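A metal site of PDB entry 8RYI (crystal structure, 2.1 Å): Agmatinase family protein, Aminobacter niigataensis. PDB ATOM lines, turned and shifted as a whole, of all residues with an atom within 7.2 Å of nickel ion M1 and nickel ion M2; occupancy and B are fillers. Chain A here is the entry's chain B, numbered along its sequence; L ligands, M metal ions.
Nickel ion M2 is bound by OD2 of Asp 202, ND1 of His 177, OD2 of Asp 206, O1 of the ligand and OD2 of Asp 295.
Nickel ion M2 has five donor atoms within binding distance.
Four residues have an atom within 4 Å of nickel ion M1: Asp 202, His 204, Asp 295 and Asp 297.
The nearest printed residue that does not touch nickel ion M1 is Cys 203 (4.4 Å).
Four residues have an atom within 4 Å of nickel ion M2: His 177, Asp 202, Asp 206 and Asp 295.
The nearest printed residue that does not touch nickel ion M2 is His 200 (4.2 Å).
The side-chain carboxylate (OD2) of Asp 297 binds nickel ion M1 (2.2 Å).
An oxygen (O1) of the ligand is bound to nickel ion M1 (2.3 Å).
Nickel ion M1 is bound by the side-chain carboxylate (OD1) of Asp 202 (2.3 Å).
Nickel ion M1 is bound by OD2 of Asp 295, at 2.4 Å.
A ring nitrogen (ND1) of His 204 binds nickel ion M1 (2.4 Å).
Nickel ion M1 is bound by OD1 of Asp 297, 2.5 Å away.
Nickel ion M1 has six donor atoms within binding distance.
Slightly farther from nickel ion M1 lies a nitrogen (N2) of the ligand (2.8 Å).
The side-chain carboxylate of Glu 339 is in hydrogen-bond range of the backbone NH of His 177 (2.7 Å).
The side-chain carboxylate (OE2) of Glu 311 sits at hydrogen-bond distance from a ring nitrogen (NE2) of His 204 (2.6 Å).
The backbone carbonyl oxygen (O) of Asp 295 lies within hydrogen-bond range of the side-chain hydroxyl (OG) of Ser 298 (2.9 Å).
O of His 204 is in hydrogen-bond range of NE2 of His 238, at 2.7 Å.
The side-chain carboxylate of Asp 202 lies close to a ring nitrogen (NE2) of His 200, at 3.0 Å.
OD2 of Asp 206 sits close to NE2 of His 200, at 3.4 Å.
OD1 of Asp 297 lies close to N of Cys 203.
O of Val 201 is in hydrogen-bond range of N of Asp 295.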
ATOM      1  N   ASP A 176      -1.450 -20.827 -17.039  1.00  0.00           N
ATOM      2  CA  ASP A 176      -1.155 -19.806 -16.040  1.00  0.00           C
ATOM      3  C   ASP A 176      -1.797 -18.477 -16.462  1.00  0.00           C
ATOM      4  O   ASP A 176      -2.364 -18.328 -17.555  1.00  0.00           O
ATOM      5  CB  ASP A 176       0.356 -19.666 -15.815  1.00  0.00           C
ATOM      6  CG  ASP A 176       1.123 -19.217 -17.064  1.00  0.00           C
ATOM      7  OD1 ASP A 176       0.668 -18.282 -17.777  1.00  0.00           O
ATOM      8  OD2 ASP A 176       2.208 -19.791 -17.340  1.00  0.00           O
ATOM      9  N   HIS A 177      -1.683 -17.481 -15.571  1.00  0.00           N
ATOM     10  CA  HIS A 177      -2.343 -16.208 -15.796  1.00  0.00           C
ATOM     11  C   HIS A 177      -1.617 -15.300 -16.778  1.00  0.00           C
ATOM     12  O   HIS A 177      -1.890 -14.087 -16.779  1.00  0.00           O
ATOM     13  CB  HIS A 177      -2.538 -15.482 -14.471  1.00  0.00           C
ATOM     14  CG  HIS A 177      -3.837 -14.745 -14.397  1.00  0.00           C
ATOM     15  ND1 HIS A 177      -4.357 -14.242 -13.214  1.00  0.00           N
ATOM     16  CD2 HIS A 177      -4.720 -14.421 -15.363  1.00  0.00           C
ATOM     17  CE1 HIS A 177      -5.503 -13.643 -13.471  1.00  0.00           C
ATOM     18  NE2 HIS A 177      -5.745 -13.742 -14.767  1.00  0.00           N
ATOM     19  N   SER A 178      -0.677 -15.814 -17.577  1.00  0.00           N
ATOM     20  CA  SER A 178      -0.229 -15.053 -18.729  1.00  0.00           C
ATOM     21  C   SER A 178      -1.295 -15.016 -19.821  1.00  0.00           C
ATOM     22  O   SER A 178      -1.202 -14.184 -20.736  1.00  0.00           O
ATOM     23  CB  SER A 178       1.086 -15.633 -19.277  1.00  0.00           C
ATOM     24  OG  SER A 178       0.931 -16.909 -19.908  1.00  0.00           O
ATOM     25  N   HIS A 200     -10.428  -8.097 -14.060  1.00  0.00           N
ATOM     26  CA  HIS A 200      -9.404  -9.016 -13.568  1.00  0.00           C
ATOM     27  C   HIS A 200      -9.815  -9.409 -12.154  1.00  0.00           C
ATOM     28  O   HIS A 200      -9.871  -8.553 -11.277  1.00  0.00           O
ATOM     29  CB  HIS A 200      -8.039  -8.324 -13.602  1.00  0.00           C
ATOM     30  CG  HIS A 200      -6.878  -9.235 -13.373  1.00  0.00           C
ATOM     31  ND1 HIS A 200      -5.922  -9.473 -14.345  1.00  0.00           N
ATOM     32  CD2 HIS A 200      -6.502  -9.957 -12.293  1.00  0.00           C
ATOM     33  CE1 HIS A 200      -5.023 -10.315 -13.876  1.00  0.00           C
ATOM     34  NE2 HIS A 200      -5.346 -10.631 -12.637  1.00  0.00           N
ATOM     35  N   VAL A 201     -10.166 -10.684 -11.932  1.00  0.00           N
ATOM     36  CA  VAL A 201     -10.636 -11.156 -10.623  1.00  0.00           C
ATOM     37  C   VAL A 201      -9.613 -12.152 -10.065  1.00  0.00           C
ATOM     38  O   VAL A 201      -9.313 -13.169 -10.695  1.00  0.00           O
ATOM     39  CB  VAL A 201     -12.038 -11.757 -10.720  1.00  0.00           C
ATOM     40  CG1 VAL A 201     -12.430 -12.359  -9.388  1.00  0.00           C
ATOM     41  CG2 VAL A 201     -13.056 -10.646 -11.118  1.00  0.00           C
ATOM     42  N   ASP A 202      -9.079 -11.857  -8.877  1.00  0.00           N
ATOM     43  CA  ASP A 202      -7.814 -12.481  -8.513  1.00  0.00           C
ATOM     44  C   ASP A 202      -7.518 -12.186  -7.055  1.00  0.00           C
ATOM     45  O   ASP A 202      -7.861 -11.119  -6.550  1.00  0.00           O
ATOM     46  CB  ASP A 202      -6.689 -11.914  -9.409  1.00  0.00           C
ATOM     47  CG  ASP A 202      -5.466 -12.820  -9.516  1.00  0.00           C
ATOM     48  OD1 ASP A 202      -5.038 -13.452  -8.544  1.00  0.00           O
ATOM     49  OD2 ASP A 202      -4.912 -12.863 -10.613  1.00  0.00           O
ATOM     50  N   CYS A 203      -6.841 -13.123  -6.391  1.00  0.00           N
ATOM     51  CA  CYS A 203      -6.315 -12.802  -5.071  1.00  0.00           C
ATOM     52  C   CYS A 203      -5.162 -11.821  -5.187  1.00  0.00           C
ATOM     53  O   CYS A 203      -4.850 -11.074  -4.244  1.00  0.00           O
ATOM     54  CB  CYS A 203      -5.838 -14.055  -4.334  1.00  0.00           C
ATOM     55  SG  CYS A 203      -5.118 -13.675  -2.709  1.00  0.00           S
ATOM     56  N   HIS A 204      -4.509 -11.825  -6.349  1.00  0.00           N
ATOM     57  CA  HIS A 204      -3.271 -11.091  -6.580  1.00  0.00           C
ATOM     58  C   HIS A 204      -3.503  -9.988  -7.595  1.00  0.00           C
ATOM     59  O   HIS A 204      -4.280 -10.146  -8.536  1.00  0.00           O
ATOM     60  CB  HIS A 204      -2.191 -12.093  -7.027  1.00  0.00           C
ATOM     61  CG  HIS A 204      -2.062 -13.259  -6.092  1.00  0.00           C
ATOM     62  ND1 HIS A 204      -2.481 -14.528  -6.415  1.00  0.00           N
ATOM     63  CD2 HIS A 204      -1.612 -13.326  -4.817  1.00  0.00           C
ATOM     64  CE1 HIS A 204      -2.279 -15.330  -5.385  1.00  0.00           C
ATOM     65  NE2 HIS A 204      -1.754 -14.627  -4.405  1.00  0.00           N
ATOM     66  N   LEU A 205      -2.825  -8.848  -7.374  1.00  0.00           N
ATOM     67  CA  LEU A 205      -3.053  -7.668  -8.201  1.00  0.00           C
ATOM     68  C   LEU A 205      -2.480  -7.816  -9.617  1.00  0.00           C
ATOM     69  O   LEU A 205      -2.925  -7.115 -10.526  1.00  0.00           O
ATOM     70  CB  LEU A 205      -2.504  -6.413  -7.475  1.00  0.00           C
ATOM     71  CG  LEU A 205      -3.252  -6.026  -6.180  1.00  0.00           C
ATOM     72  CD1 LEU A 205      -2.490  -5.053  -5.270  1.00  0.00           C
ATOM     73  CD2 LEU A 205      -4.642  -5.464  -6.514  1.00  0.00           C
ATOM     74  N   ASP A 206      -1.504  -8.734  -9.820  1.00  0.00           N
ATOM     75  CA  ASP A 206      -0.972  -9.042 -11.160  1.00  0.00           C
ATOM     76  C   ASP A 206      -0.683  -7.786 -11.990  1.00  0.00           C
ATOM     77  O   ASP A 206      -1.188  -7.612 -13.103  1.00  0.00           O
ATOM     78  CB  ASP A 206      -1.947  -9.963 -11.936  1.00  0.00           C
ATOM     79  CG  ASP A 206      -1.914 -11.413 -11.448  1.00  0.00           C
ATOM     80  OD1 ASP A 206      -1.435 -11.698 -10.335  1.00  0.00           O
ATOM     81  OD2 ASP A 206      -2.386 -12.295 -12.210  1.00  0.00           O
ATOM     82  N   ASN A 218       2.906 -14.166 -15.937  1.00  0.00           N
ATOM     83  CA  ASN A 218       1.555 -14.278 -15.418  1.00  0.00           C
ATOM     84  C   ASN A 218       1.267 -13.314 -14.284  1.00  0.00           C
ATOM     85  O   ASN A 218       0.236 -13.466 -13.621  1.00  0.00           O
ATOM     86  CB  ASN A 218       1.279 -15.726 -14.974  1.00  0.00           C
ATOM     87  CG  ASN A 218       2.096 -16.142 -13.751  1.00  0.00           C
ATOM     88  OD1 ASN A 218       3.237 -15.724 -13.560  1.00  0.00           O
ATOM     89  ND2 ASN A 218       1.500 -17.029 -12.921  1.00  0.00           N
ATOM     90  N   CYS A 219       2.123 -12.313 -14.046  1.00  0.00           N
ATOM     91  CA  CYS A 219       1.780 -11.274 -13.087  1.00  0.00           C
ATOM     92  C   CYS A 219       1.628  -9.905 -13.760  1.00  0.00           C
ATOM     93  O   CYS A 219       1.740  -8.871 -13.090  1.00  0.00           O
ATOM     94  CB  CYS A 219       2.808 -11.211 -11.954  1.00  0.00           C
ATOM     95  SG  CYS A 219       4.407 -10.477 -12.417  1.00  0.00           S
ATOM     96  N   HIS A 238     -10.166  -4.357 -10.887  1.00  0.00           N
ATOM     97  CA  HIS A 238      -9.625  -5.550 -10.259  1.00  0.00           C
ATOM     98  C   HIS A 238     -10.476  -5.874  -9.045  1.00  0.00           C
ATOM     99  O   HIS A 238     -10.832  -4.961  -8.288  1.00  0.00           O
ATOM    100  CB  HIS A 238      -8.163  -5.362  -9.856  1.00  0.00           C
ATOM    101  CG  HIS A 238      -7.483  -6.635  -9.456  1.00  0.00           C
ATOM    102  ND1 HIS A 238      -7.824  -7.334  -8.315  1.00  0.00           N
ATOM    103  CD2 HIS A 238      -6.483  -7.334 -10.046  1.00  0.00           C
ATOM    104  CE1 HIS A 238      -7.061  -8.413  -8.225  1.00  0.00           C
ATOM    105  NE2 HIS A 238      -6.232  -8.421  -9.261  1.00  0.00           N
ATOM    106  N   LEU A 245       1.002 -11.657  -0.945  1.00  0.00           N
ATOM    107  CA  LEU A 245       1.664 -11.996  -2.208  1.00  0.00           C
ATOM    108  C   LEU A 245       1.234 -10.940  -3.224  1.00  0.00           C
ATOM    109  O   LEU A 245       0.527 -11.185  -4.211  1.00  0.00           O
ATOM    110  CB  LEU A 245       1.324 -13.427  -2.653  1.00  0.00           C
ATOM    111  CG  LEU A 245       1.971 -13.924  -3.969  1.00  0.00           C
ATOM    112  CD1 LEU A 245       3.479 -13.783  -3.936  1.00  0.00           C
ATOM    113  CD2 LEU A 245       1.589 -15.375  -4.380  1.00  0.00           C
ATOM    114  N   TRP A 250       2.705  -3.635  -7.776  1.00  0.00           N
ATOM    115  CA  TRP A 250       1.407  -4.093  -8.274  1.00  0.00           C
ATOM    116  C   TRP A 250       0.275  -3.198  -7.781  1.00  0.00           C
ATOM    117  O   TRP A 250      -0.680  -2.934  -8.528  1.00  0.00           O
ATOM    118  CB  TRP A 250       1.141  -5.534  -7.849  1.00  0.00           C
ATOM    119  CG  TRP A 250       2.116  -6.575  -8.394  1.00  0.00           C
ATOM    120  CD1 TRP A 250       3.243  -6.348  -9.129  1.00  0.00           C
ATOM    121  CD2 TRP A 250       2.038  -7.991  -8.223  1.00  0.00           C
ATOM    122  NE1 TRP A 250       3.875  -7.542  -9.429  1.00  0.00           N
ATOM    123  CE2 TRP A 250       3.146  -8.566  -8.881  1.00  0.00           C
ATOM    124  CE3 TRP A 250       1.144  -8.833  -7.544  1.00  0.00           C
ATOM    125  CZ2 TRP A 250       3.384  -9.939  -8.895  1.00  0.00           C
ATOM    126  CZ3 TRP A 250       1.371 -10.189  -7.569  1.00  0.00           C
ATOM    127  CH2 TRP A 250       2.485 -10.735  -8.245  1.00  0.00           C
ATOM    128  N   THR A 293     -10.998 -11.846 -17.035  1.00  0.00           N
ATOM    129  CA  THR A 293     -10.061 -12.881 -16.614  1.00  0.00           C
ATOM    130  C   THR A 293     -10.279 -13.189 -15.136  1.00  0.00           C
ATOM    131  O   THR A 293     -10.402 -12.274 -14.306  1.00  0.00           O
ATOM    132  CB  THR A 293      -8.602 -12.498 -16.887  1.00  0.00           C
ATOM    133  OG1 THR A 293      -7.748 -13.562 -16.459  1.00  0.00           O
ATOM    134  CG2 THR A 293      -8.181 -11.219 -16.147  1.00  0.00           C
ATOM    135  N   TRP A 294     -10.352 -14.489 -14.816  1.00  0.00           N
ATOM    136  CA  TRP A 294     -10.744 -14.962 -13.495  1.00  0.00           C
ATOM    137  C   TRP A 294      -9.731 -15.981 -12.991  1.00  0.00           C
ATOM    138  O   TRP A 294      -9.692 -17.128 -13.484  1.00  0.00           O
ATOM    139  CB  TRP A 294     -12.166 -15.537 -13.533  1.00  0.00           C
ATOM    140  CG  TRP A 294     -12.827 -15.724 -12.192  1.00  0.00           C
ATOM    141  CD1 TRP A 294     -12.248 -15.571 -10.966  1.00  0.00           C
ATOM    142  CD2 TRP A 294     -14.198 -16.062 -11.954  1.00  0.00           C
ATOM    143  NE1 TRP A 294     -13.167 -15.809  -9.969  1.00  0.00           N
ATOM    144  CE2 TRP A 294     -14.379 -16.111 -10.556  1.00  0.00           C
ATOM    145  CE3 TRP A 294     -15.282 -16.350 -12.786  1.00  0.00           C
ATOM    146  CZ2 TRP A 294     -15.606 -16.453  -9.964  1.00  0.00           C
ATOM    147  CZ3 TRP A 294     -16.529 -16.670 -12.185  1.00  0.00           C
ATOM    148  CH2 TRP A 294     -16.661 -16.730 -10.791  1.00  0.00           C
ATOM    149  N   ASP A 295      -8.921 -15.587 -12.020  1.00  0.00           N
ATOM    150  CA  ASP A 295      -7.937 -16.509 -11.443  1.00  0.00           C
ATOM    151  C   ASP A 295      -8.613 -17.358 -10.369  1.00  0.00           C
ATOM    152  O   ASP A 295      -9.305 -16.831  -9.483  1.00  0.00           O
ATOM    153  CB  ASP A 295      -6.771 -15.726 -10.851  1.00  0.00           C
ATOM    154  CG  ASP A 295      -5.612 -16.603 -10.418  1.00  0.00           C
ATOM    155  OD1 ASP A 295      -5.789 -17.804 -10.055  1.00  0.00           O
ATOM    156  OD2 ASP A 295      -4.501 -16.066 -10.447  1.00  0.00           O
ATOM    157  N   THR A 296      -8.420 -18.680 -10.437  1.00  0.00           N
ATOM    158  CA  THR A 296      -9.078 -19.531  -9.442  1.00  0.00           C
ATOM    159  C   THR A 296      -8.624 -19.225  -8.021  1.00  0.00           C
ATOM    160  O   THR A 296      -9.339 -19.569  -7.083  1.00  0.00           O
ATOM    161  CB  THR A 296      -8.872 -21.036  -9.732  1.00  0.00           C
ATOM    162  OG1 THR A 296      -7.484 -21.317  -9.916  1.00  0.00           O
ATOM    163  CG2 THR A 296      -9.664 -21.455 -10.966  1.00  0.00           C
ATOM    164  N   ASP A 297      -7.464 -18.597  -7.815  1.00  0.00           N
ATOM    165  CA  ASP A 297      -7.127 -18.337  -6.414  1.00  0.00           C
ATOM    166  C   ASP A 297      -7.866 -17.136  -5.804  1.00  0.00           C
ATOM    167  O   ASP A 297      -7.677 -16.853  -4.615  1.00  0.00           O
ATOM    168  CB  ASP A 297      -5.619 -18.187  -6.219  1.00  0.00           C
ATOM    169  CG  ASP A 297      -5.028 -17.041  -6.982  1.00  0.00           C
ATOM    170  OD1 ASP A 297      -5.691 -15.977  -7.180  1.00  0.00           O
ATOM    171  OD2 ASP A 297      -3.857 -17.214  -7.382  1.00  0.00           O
ATOM    172  N   SER A 298      -8.711 -16.460  -6.580  1.00  0.00           N
ATOM    173  CA  SER A 298      -9.655 -15.557  -5.938  1.00  0.00           C
ATOM    174  C   SER A 298     -10.589 -16.328  -5.018  1.00  0.00           C
ATOM    175  O   SER A 298     -11.135 -15.754  -4.067  1.00  0.00           O
ATOM    176  CB  SER A 298     -10.476 -14.824  -7.010  1.00  0.00           C
ATOM    177  OG  SER A 298     -11.325 -15.741  -7.707  1.00  0.00           O
ATOM    178  N   ALA A 309      -1.015 -21.077  -6.274  1.00  0.00           N
ATOM    179  CA  ALA A 309      -0.884 -20.120  -5.171  1.00  0.00           C
ATOM    180  C   ALA A 309      -2.223 -19.992  -4.463  1.00  0.00           C
ATOM    181  O   ALA A 309      -2.890 -18.951  -4.542  1.00  0.00           O
ATOM    182  CB  ALA A 309      -0.405 -18.769  -5.704  1.00  0.00           C
ATOM    183  N   GLU A 311      -5.083 -19.397  -1.676  1.00  0.00           N
ATOM    184  CA  GLU A 311      -5.089 -18.350  -0.658  1.00  0.00           C
ATOM    185  C   GLU A 311      -6.346 -18.418   0.201  1.00  0.00           C
ATOM    186  O   GLU A 311      -7.444 -18.623  -0.313  1.00  0.00           O
ATOM    187  CB  GLU A 311      -5.020 -16.967  -1.308  1.00  0.00           C
ATOM    188  CG  GLU A 311      -3.749 -16.690  -2.120  1.00  0.00           C
ATOM    189  CD  GLU A 311      -2.755 -15.881  -1.298  1.00  0.00           C
ATOM    190  OE1 GLU A 311      -2.963 -15.780  -0.067  1.00  0.00           O
ATOM    191  OE2 GLU A 311      -1.802 -15.322  -1.885  1.00  0.00           O
ATOM    192  N   VAL A 338      -8.053 -19.399 -15.016  1.00  0.00           N
ATOM    193  CA  VAL A 338      -6.656 -19.820 -15.046  1.00  0.00           C
ATOM    194  C   VAL A 338      -6.224 -20.417 -13.707  1.00  0.00           C
ATOM    195  O   VAL A 338      -6.891 -20.302 -12.681  1.00  0.00           O
ATOM    196  CB  VAL A 338      -5.723 -18.643 -15.404  1.00  0.00           C
ATOM    197  CG1 VAL A 338      -6.049 -18.116 -16.783  1.00  0.00           C
ATOM    198  CG2 VAL A 338      -5.892 -17.521 -14.343  1.00  0.00           C
ATOM    199  N   GLU A 339      -5.054 -21.051 -13.763  1.00  0.00           N
ATOM    200  CA  GLU A 339      -4.227 -21.531 -12.653  1.00  0.00           C
ATOM    201  C   GLU A 339      -4.763 -22.763 -11.939  1.00  0.00           C
ATOM    202  O   GLU A 339      -4.195 -23.135 -10.910  1.00  0.00           O
ATOM    203  CB  GLU A 339      -3.953 -20.409 -11.641  1.00  0.00           C
ATOM    204  CG  GLU A 339      -3.335 -19.132 -12.290  1.00  0.00           C
ATOM    205  CD  GLU A 339      -1.804 -19.177 -12.459  1.00  0.00           C
ATOM    206  OE1 GLU A 339      -1.173 -20.194 -12.090  1.00  0.00           O
ATOM    207  OE2 GLU A 339      -1.200 -18.202 -12.967  1.00  0.00           O
HETATM  208  C1  LIG L   1      -0.992 -15.113  -9.500  1.00  0.00           C
HETATM  209  O1  LIG L   1      -1.952 -14.287  -9.594  1.00  0.00           O
HETATM  210  N1  LIG L   1       0.287 -14.711  -9.544  1.00  0.00           N
HETATM  211  N2  LIG L   1      -1.226 -16.440  -9.386  1.00  0.00           N
HETATM  212 NI    NI M   1      -3.622 -15.248  -8.406  1.00  0.00          NI
HETATM  213 NI    NI M   2      -3.332 -14.078 -11.357  1.00  0.00          NI
